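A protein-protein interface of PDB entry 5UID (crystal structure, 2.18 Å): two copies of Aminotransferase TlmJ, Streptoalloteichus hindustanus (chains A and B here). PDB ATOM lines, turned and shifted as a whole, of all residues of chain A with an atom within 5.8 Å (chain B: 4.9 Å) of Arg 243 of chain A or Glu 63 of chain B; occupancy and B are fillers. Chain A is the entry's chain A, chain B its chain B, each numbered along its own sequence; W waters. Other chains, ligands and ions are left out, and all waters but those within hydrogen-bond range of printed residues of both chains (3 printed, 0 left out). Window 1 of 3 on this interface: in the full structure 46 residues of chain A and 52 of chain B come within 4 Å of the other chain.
Glu 63 of chain A touches Arg 243 of chain B, and with the chains exchanged Arg 243 of chain A touches Glu 63 of chain B. Phe 66 of chain A touches Arg 243 of chain B, and with the chains exchanged Arg 243 of chain A touches Phe 66 of chain B. Arg 243 of chain A touches its own counterpart, Arg 243 of chain B. Of the 11 pairs that touch across the chains among the printed residues, 5 have their exchanged pair printed and touching as well.
Water W3 bridges the side-chain carboxylate (OE1) of Glu 63 of chain A and the side-chain carboxylate (OE1) of Glu 63 of chain B. Water W2 bridges the guanidinium group of Arg 243 of chain B and the guanidinium group of Arg 243 of chain A. Water W1 lies within hydrogen-bond range of O of Arg 244 of chain A, OE1 of Glu 63 of chain B and SG of Cys 60 of chain B.
Hydrophobic or aromatic side chains of chain A that line the printed part of chain B: Phe 66 and Leu 214. Among the printed residues, 11 pairs touch across the chains. Among the printed residues, no Asp or Glu carboxylate lies within 4 Å of a Lys or Arg side-chain nitrogen of the other chain.
OP1 of LLP 187 of chain B lies close to NE of Arg 244 of chain A.
Printed residues of chain B within 4 Å of Glu 63 of chain A: Arg 243 (3.7 Å). Of chain B, only Glu 63, Phe 66 and Arg 243 come within 4 Å of Arg 243 of chain A. Of the printed residues of chain A, Thr 62 of chain B touches Leu 214 and Arg 244. Glu 63 of chain B touches one residue of chain A. Of the printed residues of chain A, Arg 243 of chain B touches Glu 63, Phe 66 and Arg 243.
Glu 63 of chain A touches Arg 243 of chain B. Phe 66 of chain A touches Arg 243 of chain B (CE2 to CG, 3.4 Å). CG2 of Thr 62 of chain B touches CD2 of Leu 214 of chain A (3.7 Å). CZ of Phe 66 of chain B touches O of Phe 241 of chain A, at 3.8 Å. CZ of Phe 66 of chain B touches O of Gly 242 of chain A (3.7 Å). Glu 63 of chain B touches Arg 243 of chain A (OE1 to CD, 3.7 Å). CE2 of Phe 66 of chain B touches CG of Arg 243 of chain A, at 3.4 Å. Arg 243 of chain A touches Arg 243 of chain B (CD to CZ, 3.5 Å). Cys 60 of chain B touches Arg 244 of chain A (SG to O, 3.9 Å). N of Arg 244 of chain A touches CG2 of Thr 62 of chain B, 3.5 Å away.
OG of Ser 245 of chain A sits at hydrogen-bond distance from OE2 of Glu 63 of chain A (2.6 Å). N of Glu 63 of chain B lies within hydrogen-bond range of SG of Cys 60 of chain B, at 3.4 Å. OP2 of LLP 187 of chain B is in hydrogen-bond range of N of Cys 61 of chain B, 2.9 Å away. The side-chain carboxylate of Glu 63 of chain B lies within salt-bridge range of the guanidinium group of Arg 243 of chain B (2.8 Å). NH1 of Arg 243 of chain A is in salt-bridge range of OE2 of Glu 70 of chain A (3.1 Å). NH2 of Arg 243 of chain A is in salt-bridge range of OE2 of Glu 63 of chain A (2.7 Å).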
ATOM      1  N   GLU A  63      30.874 -31.167  20.524  1.00  0.00           N
ATOM      2  CA  GLU A  63      30.049 -30.178  21.203  1.00  0.00           C
ATOM      3  C   GLU A  63      30.900 -29.028  21.721  1.00  0.00           C
ATOM      4  O   GLU A  63      30.487 -27.865  21.665  1.00  0.00           O
ATOM      5  CB  GLU A  63      29.280 -30.840  22.343  1.00  0.00           C
ATOM      6  CG  GLU A  63      28.284 -29.929  23.020  1.00  0.00           C
ATOM      7  CD  GLU A  63      27.094 -29.600  22.144  1.00  0.00           C
ATOM      8  OE1 GLU A  63      26.854 -30.324  21.155  1.00  0.00           O
ATOM      9  OE2 GLU A  63      26.394 -28.613  22.448  1.00  0.00           O
ATOM     10  N   PHE A  66      31.540 -26.862  18.653  1.00  0.00           N
ATOM     11  CA  PHE A  66      30.363 -26.058  18.333  1.00  0.00           C
ATOM     12  C   PHE A  66      30.190 -24.915  19.326  1.00  0.00           C
ATOM     13  O   PHE A  66      29.868 -23.787  18.935  1.00  0.00           O
ATOM     14  CB  PHE A  66      29.108 -26.934  18.312  1.00  0.00           C
ATOM     15  CG  PHE A  66      28.806 -27.538  16.971  1.00  0.00           C
ATOM     16  CD1 PHE A  66      29.537 -28.616  16.495  1.00  0.00           C
ATOM     17  CD2 PHE A  66      27.771 -27.040  16.191  1.00  0.00           C
ATOM     18  CE1 PHE A  66      29.256 -29.176  15.264  1.00  0.00           C
ATOM     19  CE2 PHE A  66      27.484 -27.595  14.957  1.00  0.00           C
ATOM     20  CZ  PHE A  66      28.227 -28.666  14.493  1.00  0.00           C
ATOM     21  N   LEU A  67      30.395 -25.188  20.617  1.00  0.00           N
ATOM     22  CA  LEU A  67      30.237 -24.145  21.626  1.00  0.00           C
ATOM     23  C   LEU A  67      31.245 -23.022  21.424  1.00  0.00           C
ATOM     24  O   LEU A  67      30.904 -21.841  21.567  1.00  0.00           O
ATOM     25  CB  LEU A  67      30.379 -24.734  23.030  1.00  0.00           C
ATOM     26  CG  LEU A  67      29.238 -25.612  23.541  1.00  0.00           C
ATOM     27  CD1 LEU A  67      29.603 -26.228  24.884  1.00  0.00           C
ATOM     28  CD2 LEU A  67      27.952 -24.810  23.645  1.00  0.00           C
ATOM     29  N   GLU A  70      30.216 -20.723  18.834  1.00  0.00           N
ATOM     30  CA  GLU A  70      29.111 -19.912  19.336  1.00  0.00           C
ATOM     31  C   GLU A  70      29.621 -18.804  20.251  1.00  0.00           C
ATOM     32  O   GLU A  70      29.239 -17.637  20.103  1.00  0.00           O
ATOM     33  CB  GLU A  70      28.099 -20.792  20.072  1.00  0.00           C
ATOM     34  CG  GLU A  70      27.350 -21.767  19.177  1.00  0.00           C
ATOM     35  CD  GLU A  70      26.473 -22.724  19.964  1.00  0.00           C
ATOM     36  OE1 GLU A  70      26.309 -22.517  21.185  1.00  0.00           O
ATOM     37  OE2 GLU A  70      25.947 -23.684  19.362  1.00  0.00           O
ATOM     38  N   LEU A 211      26.092 -21.596  28.981  1.00  0.00           N
ATOM     39  CA  LEU A 211      25.616 -22.026  27.670  1.00  0.00           C
ATOM     40  C   LEU A 211      25.506 -23.545  27.590  1.00  0.00           C
ATOM     41  O   LEU A 211      24.550 -24.076  27.009  1.00  0.00           O
ATOM     42  CB  LEU A 211      26.539 -21.492  26.576  1.00  0.00           C
ATOM     43  CG  LEU A 211      26.119 -21.790  25.136  1.00  0.00           C
ATOM     44  CD1 LEU A 211      24.744 -21.202  24.852  1.00  0.00           C
ATOM     45  CD2 LEU A 211      27.145 -21.257  24.153  1.00  0.00           C
ATOM     46  N   ALA A 212      26.470 -24.262  28.173  1.00  0.00           N
ATOM     47  CA  ALA A 212      26.399 -25.719  28.194  1.00  0.00           C
ATOM     48  C   ALA A 212      25.238 -26.227  29.037  1.00  0.00           C
ATOM     49  O   ALA A 212      24.771 -27.347  28.812  1.00  0.00           O
ATOM     50  CB  ALA A 212      27.711 -26.309  28.711  1.00  0.00           C
ATOM     51  N   SER A 213      24.768 -25.437  29.995  1.00  0.00           N
ATOM     52  CA  SER A 213      23.625 -25.803  30.832  1.00  0.00           C
ATOM     53  C   SER A 213      22.352 -25.108  30.366  1.00  0.00           C
ATOM     54  O   SER A 213      21.666 -24.446  31.146  1.00  0.00           O
ATOM     55  CB  SER A 213      23.916 -25.481  32.293  1.00  0.00           C
ATOM     56  OG  SER A 213      24.884 -26.365  32.830  1.00  0.00           O
ATOM     57  N   LEU A 214      22.036 -25.247  29.077  1.00  0.00           N
ATOM     58  CA  LEU A 214      20.787 -24.764  28.486  1.00  0.00           C
ATOM     59  C   LEU A 214      20.657 -23.245  28.539  1.00  0.00           C
ATOM     60  O   LEU A 214      19.552 -22.709  28.410  1.00  0.00           O
ATOM     61  CB  LEU A 214      19.570 -25.417  29.155  1.00  0.00           C
ATOM     62  CG  LEU A 214      19.455 -26.935  29.011  1.00  0.00           C
ATOM     63  CD1 LEU A 214      18.763 -27.533  30.221  1.00  0.00           C
ATOM     64  CD2 LEU A 214      18.695 -27.287  27.743  1.00  0.00           C
ATOM     65  N   GLY A 215      21.769 -22.534  28.717  1.00  0.00           N
ATOM     66  CA  GLY A 215      21.714 -21.089  28.837  1.00  0.00           C
ATOM     67  C   GLY A 215      21.056 -20.575  30.097  1.00  0.00           C
ATOM     68  O   GLY A 215      20.752 -19.382  30.176  1.00  0.00           O
ATOM     69  N   PHE A 241      19.729 -19.610  24.074  1.00  0.00           N
ATOM     70  CA  PHE A 241      18.950 -20.789  23.694  1.00  0.00           C
ATOM     71  C   PHE A 241      19.866 -22.008  23.554  1.00  0.00           C
ATOM     72  O   PHE A 241      19.987 -22.627  22.496  1.00  0.00           O
ATOM     73  CB  PHE A 241      18.180 -20.509  22.408  1.00  0.00           C
ATOM     74  CG  PHE A 241      17.278 -19.307  22.490  1.00  0.00           C
ATOM     75  CD1 PHE A 241      16.426 -19.136  23.570  1.00  0.00           C
ATOM     76  CD2 PHE A 241      17.293 -18.343  21.495  1.00  0.00           C
ATOM     77  CE1 PHE A 241      15.597 -18.030  23.651  1.00  0.00           C
ATOM     78  CE2 PHE A 241      16.468 -17.235  21.570  1.00  0.00           C
ATOM     79  CZ  PHE A 241      15.618 -17.079  22.651  1.00  0.00           C
ATOM     80  N   GLY A 242      20.514 -22.356  24.668  1.00  0.00           N
ATOM     81  CA  GLY A 242      21.534 -23.378  24.639  1.00  0.00           C
ATOM     82  C   GLY A 242      20.982 -24.790  24.696  1.00  0.00           C
ATOM     83  O   GLY A 242      19.875 -25.047  25.173  1.00  0.00           O
ATOM     84  N   ARG A 243      21.785 -25.721  24.184  1.00  0.00           N
ATOM     85  CA  ARG A 243      21.505 -27.145  24.302  1.00  0.00           C
ATOM     86  C   ARG A 243      21.933 -27.621  25.688  1.00  0.00           C
ATOM     87  O   ARG A 243      22.348 -26.833  26.543  1.00  0.00           O
ATOM     88  CB  ARG A 243      22.217 -27.923  23.196  1.00  0.00           C
ATOM     89  CG  ARG A 243      21.803 -27.536  21.788  1.00  0.00           C
ATOM     90  CD  ARG A 243      22.620 -28.271  20.734  1.00  0.00           C
ATOM     91  NE  ARG A 243      24.049 -28.006  20.878  1.00  0.00           N
ATOM     92  CZ  ARG A 243      24.679 -26.974  20.324  1.00  0.00           C
ATOM     93  NH1 ARG A 243      24.008 -26.102  19.582  1.00  0.00           N
ATOM     94  NH2 ARG A 243      25.981 -26.813  20.512  1.00  0.00           N
ATOM     95  N   ARG A 244      21.838 -28.926  25.927  1.00  0.00           N
ATOM     96  CA  ARG A 244      22.361 -29.545  27.143  1.00  0.00           C
ATOM     97  C   ARG A 244      23.671 -30.222  26.757  1.00  0.00           C
ATOM     98  O   ARG A 244      23.675 -31.276  26.115  1.00  0.00           O
ATOM     99  CB  ARG A 244      21.358 -30.530  27.735  1.00  0.00           C
ATOM    100  CG  ARG A 244      21.706 -31.018  29.136  1.00  0.00           C
ATOM    101  CD  ARG A 244      20.605 -31.910  29.675  1.00  0.00           C
ATOM    102  NE  ARG A 244      20.898 -32.459  30.999  1.00  0.00           N
ATOM    103  CZ  ARG A 244      21.511 -33.620  31.209  1.00  0.00           C
ATOM    104  NH1 ARG A 244      21.911 -34.355  30.179  1.00  0.00           N
ATOM    105  NH2 ARG A 244      21.722 -34.053  32.447  1.00  0.00           N
ATOM    106  N   SER A 245      24.785 -29.608  27.148  1.00  0.00           N
ATOM    107  CA  SER A 245      26.103 -29.976  26.647  1.00  0.00           C
ATOM    108  C   SER A 245      27.033 -30.435  27.766  1.00  0.00           C
ATOM    109  O   SER A 245      28.253 -30.324  27.649  1.00  0.00           O
ATOM    110  CB  SER A 245      26.723 -28.801  25.894  1.00  0.00           C
ATOM    111  OG  SER A 245      25.821 -28.279  24.934  1.00  0.00           O
ATOM    112  N   SER B  59      22.314 -38.732  22.375  1.00  0.00           N
ATOM    113  CA  SER B  59      23.107 -38.464  23.570  1.00  0.00           C
ATOM    114  C   SER B  59      22.244 -38.028  24.749  1.00  0.00           C
ATOM    115  O   SER B  59      22.575 -38.335  25.901  1.00  0.00           O
ATOM    116  CB  SER B  59      24.167 -37.405  23.272  1.00  0.00           C
ATOM    117  OG  SER B  59      23.569 -36.194  22.843  1.00  0.00           O
ATOM    118  N   CYS B  60      21.150 -37.315  24.493  1.00  0.00           N
ATOM    119  CA  CYS B  60      20.235 -36.912  25.553  1.00  0.00           C
ATOM    120  C   CYS B  60      18.917 -36.482  24.924  1.00  0.00           C
ATOM    121  O   CYS B  60      18.805 -36.341  23.703  1.00  0.00           O
ATOM    122  CB  CYS B  60      20.828 -35.790  26.413  1.00  0.00           C
ATOM    123  SG  CYS B  60      21.258 -34.288  25.506  1.00  0.00           S
ATOM    124  N   CYS B  61      17.915 -36.274  25.782  1.00  0.00           N
ATOM    125  CA  CYS B  61      16.595 -35.880  25.298  1.00  0.00           C
ATOM    126  C   CYS B  61      16.604 -34.458  24.751  1.00  0.00           C
ATOM    127  O   CYS B  61      15.900 -34.159  23.779  1.00  0.00           O
ATOM    128  CB  CYS B  61      15.563 -36.013  26.415  1.00  0.00           C
ATOM    129  SG  CYS B  61      13.873 -35.551  25.947  1.00  0.00           S
ATOM    130  N   THR B  62      17.376 -33.563  25.375  1.00  0.00           N
ATOM    131  CA  THR B  62      17.507 -32.208  24.846  1.00  0.00           C
ATOM    132  C   THR B  62      18.027 -32.233  23.416  1.00  0.00           C
ATOM    133  O   THR B  62      17.501 -31.536  22.541  1.00  0.00           O
ATOM    134  CB  THR B  62      18.438 -31.379  25.730  1.00  0.00           C
ATOM    135  OG1 THR B  62      17.928 -31.336  27.070  1.00  0.00           O
ATOM    136  CG2 THR B  62      18.567 -29.959  25.188  1.00  0.00           C
ATOM    137  N   GLU B  63      19.058 -33.041  23.163  1.00  0.00           N
ATOM    138  CA  GLU B  63      19.586 -33.169  21.811  1.00  0.00           C
ATOM    139  C   GLU B  63      18.538 -33.744  20.867  1.00  0.00           C
ATOM    140  O   GLU B  63      18.407 -33.290  19.725  1.00  0.00           O
ATOM    141  CB  GLU B  63      20.841 -34.040  21.827  1.00  0.00           C
ATOM    142  CG  GLU B  63      21.599 -34.055  20.517  1.00  0.00           C
ATOM    143  CD  GLU B  63      22.368 -32.772  20.264  1.00  0.00           C
ATOM    144  OE1 GLU B  63      22.407 -31.906  21.163  1.00  0.00           O
ATOM    145  OE2 GLU B  63      22.939 -32.632  19.163  1.00  0.00           O
ATOM    146  N   GLY B  64      17.776 -34.737  21.330  1.00  0.00           N
ATOM    147  CA  GLY B  64      16.672 -35.238  20.528  1.00  0.00           C
ATOM    148  C   GLY B  64      15.658 -34.160  20.195  1.00  0.00           C
ATOM    149  O   GLY B  64      15.165 -34.084  19.066  1.00  0.00           O
ATOM    150  N   LEU B  65      15.340 -33.303  21.167  1.00  0.00           N
ATOM    151  CA  LEU B  65      14.395 -32.221  20.909  1.00  0.00           C
ATOM    152  C   LEU B  65      14.960 -31.228  19.901  1.00  0.00           C
ATOM    153  O   LEU B  65      14.237 -30.755  19.016  1.00  0.00           O
ATOM    154  CB  LEU B  65      14.028 -31.520  22.217  1.00  0.00           C
ATOM    155  CG  LEU B  65      13.141 -32.328  23.171  1.00  0.00           C
ATOM    156  CD1 LEU B  65      13.090 -31.692  24.553  1.00  0.00           C
ATOM    157  CD2 LEU B  65      11.740 -32.458  22.590  1.00  0.00           C
ATOM    158  N   PHE B  66      16.253 -30.906  20.015  1.00  0.00           N
ATOM    159  CA  PHE B  66      16.882 -30.009  19.051  1.00  0.00           C
ATOM    160  C   PHE B  66      16.893 -30.620  17.656  1.00  0.00           C
ATOM    161  O   PHE B  66      16.601 -29.934  16.668  1.00  0.00           O
ATOM    162  CB  PHE B  66      18.307 -29.666  19.499  1.00  0.00           C
ATOM    163  CG  PHE B  66      18.404 -28.412  20.332  1.00  0.00           C
ATOM    164  CD1 PHE B  66      18.056 -28.422  21.675  1.00  0.00           C
ATOM    165  CD2 PHE B  66      18.855 -27.225  19.769  1.00  0.00           C
ATOM    166  CE1 PHE B  66      18.145 -27.269  22.442  1.00  0.00           C
ATOM    167  CE2 PHE B  66      18.948 -26.066  20.530  1.00  0.00           C
ATOM    168  CZ  PHE B  66      18.593 -26.087  21.868  1.00  0.00           C
ATOM    169  N   LEU B  67      17.224 -31.910  17.555  1.00  0.00           N
ATOM    170  CA  LEU B  67      17.276 -32.563  16.250  1.00  0.00           C
ATOM    171  C   LEU B  67      15.908 -32.581  15.581  1.00  0.00           C
ATOM    172  O   LEU B  67      15.804 -32.427  14.359  1.00  0.00           O
ATOM    173  CB  LEU B  67      17.815 -33.987  16.392  1.00  0.00           C
ATOM    174  CG  LEU B  67      19.286 -34.167  16.773  1.00  0.00           C
ATOM    175  CD1 LEU B  67      19.595 -35.638  17.017  1.00  0.00           C
ATOM    176  CD2 LEU B  67      20.206 -33.595  15.704  1.00  0.00           C
ATOM    177  N1  LLP B 187      12.302 -33.156  29.011  1.00  0.00           N
ATOM    178  C2  LLP B 187      11.715 -33.419  30.184  1.00  0.00           C
ATOM    179  C2' LLP B 187      10.160 -33.409  30.297  1.00  0.00           C
ATOM    180  C3  LLP B 187      12.502 -33.717  31.329  1.00  0.00           C
ATOM    181  O3  LLP B 187      11.879 -33.995  32.552  1.00  0.00           O
ATOM    182  C4  LLP B 187      13.876 -33.732  31.240  1.00  0.00           C
ATOM    183  C4' LLP B 187      14.768 -34.069  32.549  1.00  0.00           C
ATOM    184  C5  LLP B 187      14.473 -33.457  30.046  1.00  0.00           C
ATOM    185  C6  LLP B 187      13.698 -33.169  28.913  1.00  0.00           C
ATOM    186  C5' LLP B 187      16.026 -33.463  29.927  1.00  0.00           C
ATOM    187  OP4 LLP B 187      16.454 -34.670  29.347  1.00  0.00           O
ATOM    188  P   LLP B 187      17.955 -34.801  29.028  1.00  0.00           P
ATOM    189  OP1 LLP B 187      18.775 -34.389  30.254  1.00  0.00           O
ATOM    190  OP2 LLP B 187      18.233 -36.214  28.687  1.00  0.00           O
ATOM    191  OP3 LLP B 187      18.304 -33.909  27.891  1.00  0.00           O
ATOM    192  N   LLP B 187      15.781 -39.383  35.788  1.00  0.00           N
ATOM    193  CA  LLP B 187      14.604 -40.087  35.237  1.00  0.00           C
ATOM    194  CB  LLP B 187      14.714 -40.193  33.732  1.00  0.00           C
ATOM    195  CG  LLP B 187      15.147 -38.867  33.088  1.00  0.00           C
ATOM    196  CD  LLP B 187      14.174 -37.711  33.397  1.00  0.00           C
ATOM    197  CE  LLP B 187      14.604 -36.463  32.584  1.00  0.00           C
ATOM    198  NZ  LLP B 187      14.233 -35.205  33.256  1.00  0.00           N
ATOM    199  C   LLP B 187      14.451 -41.446  35.856  1.00  0.00           C
ATOM    200  O   LLP B 187      14.970 -41.697  36.934  1.00  0.00           O
ATOM    201  N   ARG B 243      26.004 -31.957  14.447  1.00  0.00           N
ATOM    202  CA  ARG B 243      26.846 -32.179  15.613  1.00  0.00           C
ATOM    203  C   ARG B 243      27.064 -33.680  15.781  1.00  0.00           C
ATOM    204  O   ARG B 243      26.675 -34.490  14.933  1.00  0.00           O
ATOM    205  CB  ARG B 243      26.213 -31.560  16.858  1.00  0.00           C
ATOM    206  CG  ARG B 243      25.906 -30.081  16.739  1.00  0.00           C
ATOM    207  CD  ARG B 243      25.159 -29.574  17.963  1.00  0.00           C
ATOM    208  NE  ARG B 243      23.873 -30.248  18.126  1.00  0.00           N
ATOM    209  CZ  ARG B 243      22.726 -29.799  17.624  1.00  0.00           C
ATOM    210  NH1 ARG B 243      22.703 -28.670  16.928  1.00  0.00           N
ATOM    211  NH2 ARG B 243      21.603 -30.476  17.822  1.00  0.00           N
ATOM    212  N   SER B 245      25.678 -36.360  17.932  1.00  0.00           N
ATOM    213  CA  SER B 245      24.505 -36.483  18.786  1.00  0.00           C
ATOM    214  C   SER B 245      24.203 -37.926  19.170  1.00  0.00           C
ATOM    215  O   SER B 245      23.055 -38.249  19.487  1.00  0.00           O
ATOM    216  CB  SER B 245      23.294 -35.863  18.087  1.00  0.00           C
ATOM    217  OG  SER B 245      23.595 -34.568  17.593  1.00  0.00           O
HETATM  218  O   HOH W   1      21.871 -31.396  23.938  1.00  0.00           O
HETATM  219  O   HOH W   2      24.107 -26.403  16.122  1.00  0.00           O
HETATM  220  O   HOH W   3      24.948 -31.800  21.907  1.00  0.00           O
